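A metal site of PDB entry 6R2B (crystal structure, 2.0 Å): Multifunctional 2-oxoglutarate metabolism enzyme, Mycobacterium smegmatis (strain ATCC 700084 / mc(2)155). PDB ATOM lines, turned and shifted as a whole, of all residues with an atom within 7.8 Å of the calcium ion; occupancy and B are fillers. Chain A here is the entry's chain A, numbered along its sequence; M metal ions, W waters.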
ATOM      1  N   GLN A 466     -12.518 -28.553  24.806  1.00  0.00           N
ATOM      2  CA  GLN A 466     -12.586 -29.198  23.502  1.00  0.00           C
ATOM      3  C   GLN A 466     -11.190 -29.482  23.006  1.00  0.00           C
ATOM      4  O   GLN A 466     -10.373 -28.578  22.876  1.00  0.00           O
ATOM      5  CB  GLN A 466     -13.366 -28.318  22.508  1.00  0.00           C
ATOM      6  CG  GLN A 466     -14.792 -28.025  22.928  1.00  0.00           C
ATOM      7  CD  GLN A 466     -15.571 -27.487  21.765  1.00  0.00           C
ATOM      8  OE1 GLN A 466     -15.965 -28.243  20.857  1.00  0.00           O
ATOM      9  NE2 GLN A 466     -15.807 -26.182  21.751  1.00  0.00           N
ATOM     10  N   LYS A 535     -21.641 -35.839   4.974  1.00  0.00           N
ATOM     11  CA  LYS A 535     -21.765 -34.535   5.647  1.00  0.00           C
ATOM     12  C   LYS A 535     -22.566 -33.513   4.858  1.00  0.00           C
ATOM     13  O   LYS A 535     -22.445 -33.410   3.626  1.00  0.00           O
ATOM     14  CB  LYS A 535     -20.380 -33.954   5.956  1.00  0.00           C
ATOM     15  CG  LYS A 535     -20.365 -33.055   7.188  1.00  0.00           C
ATOM     16  CD  LYS A 535     -18.961 -32.617   7.533  1.00  0.00           C
ATOM     17  CE  LYS A 535     -18.924 -31.811   8.802  1.00  0.00           C
ATOM     18  NZ  LYS A 535     -19.243 -32.646   9.997  1.00  0.00           N
ATOM     19  N   PRO A 608     -24.535 -28.741  14.618  1.00  0.00           N
ATOM     20  CA  PRO A 608     -23.089 -28.960  14.830  1.00  0.00           C
ATOM     21  C   PRO A 608     -22.418 -29.950  13.859  1.00  0.00           C
ATOM     22  O   PRO A 608     -21.187 -29.912  13.699  1.00  0.00           O
ATOM     23  CB  PRO A 608     -23.028 -29.524  16.254  1.00  0.00           C
ATOM     24  CG  PRO A 608     -24.304 -29.127  16.882  1.00  0.00           C
ATOM     25  CD  PRO A 608     -25.323 -29.075  15.824  1.00  0.00           C
ATOM     26  N   ALA A 610     -23.025 -30.052  10.600  1.00  0.00           N
ATOM     27  CA  ALA A 610     -22.868 -29.415   9.309  1.00  0.00           C
ATOM     28  C   ALA A 610     -21.489 -28.735   9.174  1.00  0.00           C
ATOM     29  O   ALA A 610     -20.924 -28.248  10.159  1.00  0.00           O
ATOM     30  CB  ALA A 610     -23.976 -28.385   9.112  1.00  0.00           C
ATOM     31  N   MET A 611     -20.968 -28.700   7.940  1.00  0.00           N
ATOM     32  CA  MET A 611     -19.778 -27.944   7.553  1.00  0.00           C
ATOM     33  C   MET A 611     -20.358 -26.620   7.008  1.00  0.00           C
ATOM     34  O   MET A 611     -21.145 -26.666   6.069  1.00  0.00           O
ATOM     35  CB  MET A 611     -18.943 -28.711   6.510  1.00  0.00           C
ATOM     36  CG  MET A 611     -17.690 -27.982   6.058  1.00  0.00           C
ATOM     37  SD  MET A 611     -16.328 -28.167   7.230  1.00  0.00           S
ATOM     38  CE  MET A 611     -15.049 -27.308   6.365  1.00  0.00           C
ATOM     39  N   SER A 644     -20.044 -22.968  18.146  1.00  0.00           N
ATOM     40  CA  SER A 644     -20.210 -22.790  16.706  1.00  0.00           C
ATOM     41  C   SER A 644     -18.973 -23.268  15.978  1.00  0.00           C
ATOM     42  O   SER A 644     -17.874 -23.061  16.465  1.00  0.00           O
ATOM     43  CB  SER A 644     -20.505 -21.341  16.360  1.00  0.00           C
ATOM     44  OG  SER A 644     -20.681 -21.208  14.962  1.00  0.00           O
ATOM     45  N   ASP A 645     -19.155 -23.910  14.834  1.00  0.00           N
ATOM     46  CA  ASP A 645     -18.059 -24.406  14.008  1.00  0.00           C
ATOM     47  C   ASP A 645     -17.989 -23.634  12.682  1.00  0.00           C
ATOM     48  O   ASP A 645     -17.428 -24.126  11.716  1.00  0.00           O
ATOM     49  CB  ASP A 645     -18.254 -25.919  13.750  1.00  0.00           C
ATOM     50  CG  ASP A 645     -16.960 -26.718  13.632  1.00  0.00           C
ATOM     51  OD1 ASP A 645     -16.001 -26.393  14.362  1.00  0.00           O
ATOM     52  OD2 ASP A 645     -16.922 -27.666  12.830  1.00  0.00           O
ATOM     53  N   VAL A 646     -18.560 -22.405  12.639  1.00  0.00           N
ATOM     54  CA  VAL A 646     -18.591 -21.603  11.417  1.00  0.00           C
ATOM     55  C   VAL A 646     -17.173 -21.325  10.883  1.00  0.00           C
ATOM     56  O   VAL A 646     -16.237 -21.122  11.658  1.00  0.00           O
ATOM     57  CB  VAL A 646     -19.420 -20.284  11.577  1.00  0.00           C
ATOM     58  CG1 VAL A 646     -18.751 -19.288  12.532  1.00  0.00           C
ATOM     59  CG2 VAL A 646     -19.740 -19.643  10.233  1.00  0.00           C
ATOM     60  N   VAL A 647     -17.025 -21.369   9.555  1.00  0.00           N
ATOM     61  CA  VAL A 647     -15.790 -21.019   8.876  1.00  0.00           C
ATOM     62  C   VAL A 647     -15.970 -19.665   8.210  1.00  0.00           C
ATOM     63  O   VAL A 647     -16.982 -19.445   7.523  1.00  0.00           O
ATOM     64  CB  VAL A 647     -15.342 -22.082   7.826  1.00  0.00           C
ATOM     65  CG1 VAL A 647     -13.973 -21.728   7.223  1.00  0.00           C
ATOM     66  CG2 VAL A 647     -15.323 -23.490   8.415  1.00  0.00           C
ATOM     67  N   LEU A 693      -9.526 -27.852   5.995  1.00  0.00           N
ATOM     68  CA  LEU A 693     -10.992 -27.931   5.935  1.00  0.00           C
ATOM     69  C   LEU A 693     -11.504 -29.284   6.384  1.00  0.00           C
ATOM     70  O   LEU A 693     -12.493 -29.349   7.107  1.00  0.00           O
ATOM     71  CB  LEU A 693     -11.504 -27.626   4.518  1.00  0.00           C
ATOM     72  CG  LEU A 693     -11.354 -26.185   4.027  1.00  0.00           C
ATOM     73  CD1 LEU A 693     -11.930 -26.075   2.621  1.00  0.00           C
ATOM     74  CD2 LEU A 693     -12.060 -25.212   4.951  1.00  0.00           C
ATOM     75  N   ARG A 694     -10.813 -30.363   5.987  1.00  0.00           N
ATOM     76  CA  ARG A 694     -11.233 -31.720   6.390  1.00  0.00           C
ATOM     77  C   ARG A 694     -11.045 -31.921   7.882  1.00  0.00           C
ATOM     78  O   ARG A 694     -11.954 -32.470   8.513  1.00  0.00           O
ATOM     79  CB  ARG A 694     -10.494 -32.787   5.589  1.00  0.00           C
ATOM     80  CG  ARG A 694     -11.126 -32.889   4.201  1.00  0.00           C
ATOM     81  CD  ARG A 694     -10.676 -34.040   3.359  1.00  0.00           C
ATOM     82  NE  ARG A 694     -10.708 -35.349   4.023  1.00  0.00           N
ATOM     83  CZ  ARG A 694     -11.777 -36.128   4.155  1.00  0.00           C
ATOM     84  NH1 ARG A 694     -12.961 -35.721   3.711  1.00  0.00           N
ATOM     85  NH2 ARG A 694     -11.666 -37.307   4.727  1.00  0.00           N
ATOM     86  N   ARG A 695      -9.925 -31.432   8.475  1.00  0.00           N
ATOM     87  CA  ARG A 695      -9.686 -31.541   9.932  1.00  0.00           C
ATOM     88  C   ARG A 695     -10.803 -30.822  10.688  1.00  0.00           C
ATOM     89  O   ARG A 695     -11.369 -31.370  11.626  1.00  0.00           O
ATOM     90  CB  ARG A 695      -8.306 -30.972  10.321  1.00  0.00           C
ATOM     91  CG  ARG A 695      -7.970 -31.078  11.815  1.00  0.00           C
ATOM     92  CD  ARG A 695      -6.654 -30.400  12.188  1.00  0.00           C
ATOM     93  NE  ARG A 695      -6.713 -28.946  12.015  1.00  0.00           N
ATOM     94  CZ  ARG A 695      -5.777 -28.098  12.430  1.00  0.00           C
ATOM     95  NH1 ARG A 695      -4.705 -28.544  13.071  1.00  0.00           N
ATOM     96  NH2 ARG A 695      -5.917 -26.802  12.214  1.00  0.00           N
ATOM     97  N   HIS A 696     -11.154 -29.614  10.231  1.00  0.00           N
ATOM     98  CA  HIS A 696     -12.211 -28.779  10.800  1.00  0.00           C
ATOM     99  C   HIS A 696     -13.578 -29.481  10.787  1.00  0.00           C
ATOM    100  O   HIS A 696     -14.319 -29.408  11.767  1.00  0.00           O
ATOM    101  CB  HIS A 696     -12.283 -27.439  10.054  1.00  0.00           C
ATOM    102  CG  HIS A 696     -13.260 -26.511  10.685  1.00  0.00           C
ATOM    103  ND1 HIS A 696     -13.008 -25.932  11.926  1.00  0.00           N
ATOM    104  CD2 HIS A 696     -14.503 -26.147  10.281  1.00  0.00           C
ATOM    105  CE1 HIS A 696     -14.095 -25.211  12.203  1.00  0.00           C
ATOM    106  NE2 HIS A 696     -14.999 -25.305  11.229  1.00  0.00           N
ATOM    107  N   GLY A 697     -13.913 -30.136   9.686  1.00  0.00           N
ATOM    108  CA  GLY A 697     -15.195 -30.824   9.573  1.00  0.00           C
ATOM    109  C   GLY A 697     -15.298 -32.139  10.317  1.00  0.00           C
ATOM    110  O   GLY A 697     -16.399 -32.540  10.720  1.00  0.00           O
ATOM    111  N   LYS A 698     -14.178 -32.832  10.498  1.00  0.00           N
ATOM    112  CA  LYS A 698     -14.139 -34.179  11.092  1.00  0.00           C
ATOM    113  C   LYS A 698     -13.592 -34.255  12.520  1.00  0.00           C
ATOM    114  O   LYS A 698     -13.586 -35.347  13.097  1.00  0.00           O
ATOM    115  CB  LYS A 698     -13.224 -35.079  10.216  1.00  0.00           C
ATOM    116  CG  LYS A 698     -13.700 -35.260   8.767  1.00  0.00           C
ATOM    117  CD  LYS A 698     -12.640 -35.928   7.900  1.00  0.00           C
ATOM    118  CE  LYS A 698     -12.490 -37.420   8.129  1.00  0.00           C
ATOM    119  NZ  LYS A 698     -13.751 -38.155   7.855  1.00  0.00           N
ATOM    120  N   ASP A 699     -13.107 -33.147  13.101  1.00  0.00           N
ATOM    121  CA  ASP A 699     -12.484 -33.220  14.439  1.00  0.00           C
ATOM    122  C   ASP A 699     -13.450 -33.396  15.618  1.00  0.00           C
ATOM    123  O   ASP A 699     -12.998 -33.697  16.716  1.00  0.00           O
ATOM    124  CB  ASP A 699     -11.557 -32.014  14.707  1.00  0.00           C
ATOM    125  CG  ASP A 699     -12.181 -30.632  14.606  1.00  0.00           C
ATOM    126  OD1 ASP A 699     -13.425 -30.532  14.572  1.00  0.00           O
ATOM    127  OD2 ASP A 699     -11.416 -29.646  14.589  1.00  0.00           O
ATOM    128  N   GLY A 700     -14.749 -33.201  15.415  1.00  0.00           N
ATOM    129  CA  GLY A 700     -15.725 -33.317  16.504  1.00  0.00           C
ATOM    130  C   GLY A 700     -15.717 -32.152  17.499  1.00  0.00           C
ATOM    131  O   GLY A 700     -16.448 -32.178  18.488  1.00  0.00           O
ATOM    132  N   ILE A 701     -14.878 -31.114  17.228  1.00  0.00           N
ATOM    133  CA  ILE A 701     -14.728 -29.863  17.995  1.00  0.00           C
ATOM    134  C   ILE A 701     -15.635 -28.838  17.335  1.00  0.00           C
ATOM    135  O   ILE A 701     -15.690 -28.790  16.112  1.00  0.00           O
ATOM    136  CB  ILE A 701     -13.240 -29.375  17.977  1.00  0.00           C
ATOM    137  CG1 ILE A 701     -12.253 -30.426  18.512  1.00  0.00           C
ATOM    138  CG2 ILE A 701     -13.056 -28.028  18.711  1.00  0.00           C
ATOM    139  CD1 ILE A 701     -10.842 -30.184  17.960  1.00  0.00           C
ATOM    140  N   GLN A 702     -16.324 -28.010  18.147  1.00  0.00           N
ATOM    141  CA  GLN A 702     -17.193 -26.973  17.618  1.00  0.00           C
ATOM    142  C   GLN A 702     -16.581 -25.620  17.964  1.00  0.00           C
ATOM    143  O   GLN A 702     -16.863 -25.062  19.039  1.00  0.00           O
ATOM    144  CB  GLN A 702     -18.635 -27.124  18.163  1.00  0.00           C
ATOM    145  CG  GLN A 702     -19.292 -28.514  17.953  1.00  0.00           C
ATOM    146  CD  GLN A 702     -19.309 -28.931  16.497  1.00  0.00           C
ATOM    147  OE1 GLN A 702     -19.862 -28.228  15.641  1.00  0.00           O
ATOM    148  NE2 GLN A 702     -18.699 -30.086  16.195  1.00  0.00           N
ATOM    149  N   ARG A 703     -15.658 -25.148  17.098  1.00  0.00           N
ATOM    150  CA  ARG A 703     -14.936 -23.870  17.290  1.00  0.00           C
ATOM    151  C   ARG A 703     -14.699 -23.197  15.948  1.00  0.00           C
ATOM    152  O   ARG A 703     -14.307 -23.872  14.994  1.00  0.00           O
ATOM    153  CB  ARG A 703     -13.632 -24.053  18.065  1.00  0.00           C
ATOM    154  CG  ARG A 703     -13.860 -24.387  19.514  1.00  0.00           C
ATOM    155  CD  ARG A 703     -12.585 -24.430  20.328  1.00  0.00           C
ATOM    156  NE  ARG A 703     -12.907 -24.453  21.760  1.00  0.00           N
ATOM    157  CZ  ARG A 703     -12.084 -24.873  22.707  1.00  0.00           C
ATOM    158  NH1 ARG A 703     -10.862 -25.289  22.403  1.00  0.00           N
ATOM    159  NH2 ARG A 703     -12.479 -24.886  23.962  1.00  0.00           N
ATOM    160  N   PRO A 704     -14.981 -21.876  15.816  1.00  0.00           N
ATOM    161  CA  PRO A 704     -14.860 -21.230  14.505  1.00  0.00           C
ATOM    162  C   PRO A 704     -13.463 -21.304  13.895  1.00  0.00           C
ATOM    163  O   PRO A 704     -12.455 -21.463  14.586  1.00  0.00           O
ATOM    164  CB  PRO A 704     -15.246 -19.783  14.791  1.00  0.00           C
ATOM    165  CG  PRO A 704     -16.098 -19.849  16.008  1.00  0.00           C
ATOM    166  CD  PRO A 704     -15.490 -20.932  16.833  1.00  0.00           C
ATOM    167  N   LEU A 705     -13.433 -21.243  12.572  1.00  0.00           N
ATOM    168  CA  LEU A 705     -12.195 -21.278  11.804  1.00  0.00           C
ATOM    169  C   LEU A 705     -12.154 -20.033  10.933  1.00  0.00           C
ATOM    170  O   LEU A 705     -13.078 -19.798  10.171  1.00  0.00           O
ATOM    171  CB  LEU A 705     -12.114 -22.575  10.947  1.00  0.00           C
ATOM    172  CG  LEU A 705     -10.970 -22.686   9.900  1.00  0.00           C
ATOM    173  CD1 LEU A 705      -9.572 -22.726  10.557  1.00  0.00           C
ATOM    174  CD2 LEU A 705     -11.162 -23.908   9.013  1.00  0.00           C
HETATM  175 CA    CA M   1     -15.027 -28.741  13.911  1.00  0.00          CA
HETATM  176  O   HOH W   1     -16.563 -30.656  13.846  1.00  0.00           O
HETATM  177  O   HOH W   2     -13.038 -27.576  14.473  1.00  0.00           O
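Water W1 lies within hydrogen-bond range of the side-chain amide nitrogen of Gln 702 (3.2 Å) and the backbone NH of Gly 700 (3.5 Å).
Water W2 lies within hydrogen-bond range of OD2 of Asp 699 (2.6 Å) and ND1 of His 696 (3.0 Å).
OD1 of Asp 645 sits close to N of Arg 703, at 3.0 Å.
The calcium ion is bound by O of Ile 701 (2.3 Å), O of His 696 (2.4 Å), water W2 (2.4 Å), OD2 of Asp 645 (2.4 Å), water W1 (2.5 Å), OD1 of Asp 699 (2.5 Å) and OD1 of Asp 645 (2.6 Å).
The calcium ion has seven donor atoms within binding distance.
The nearest printed residue that does not touch the calcium ion is Gln 702 (4.5 Å).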
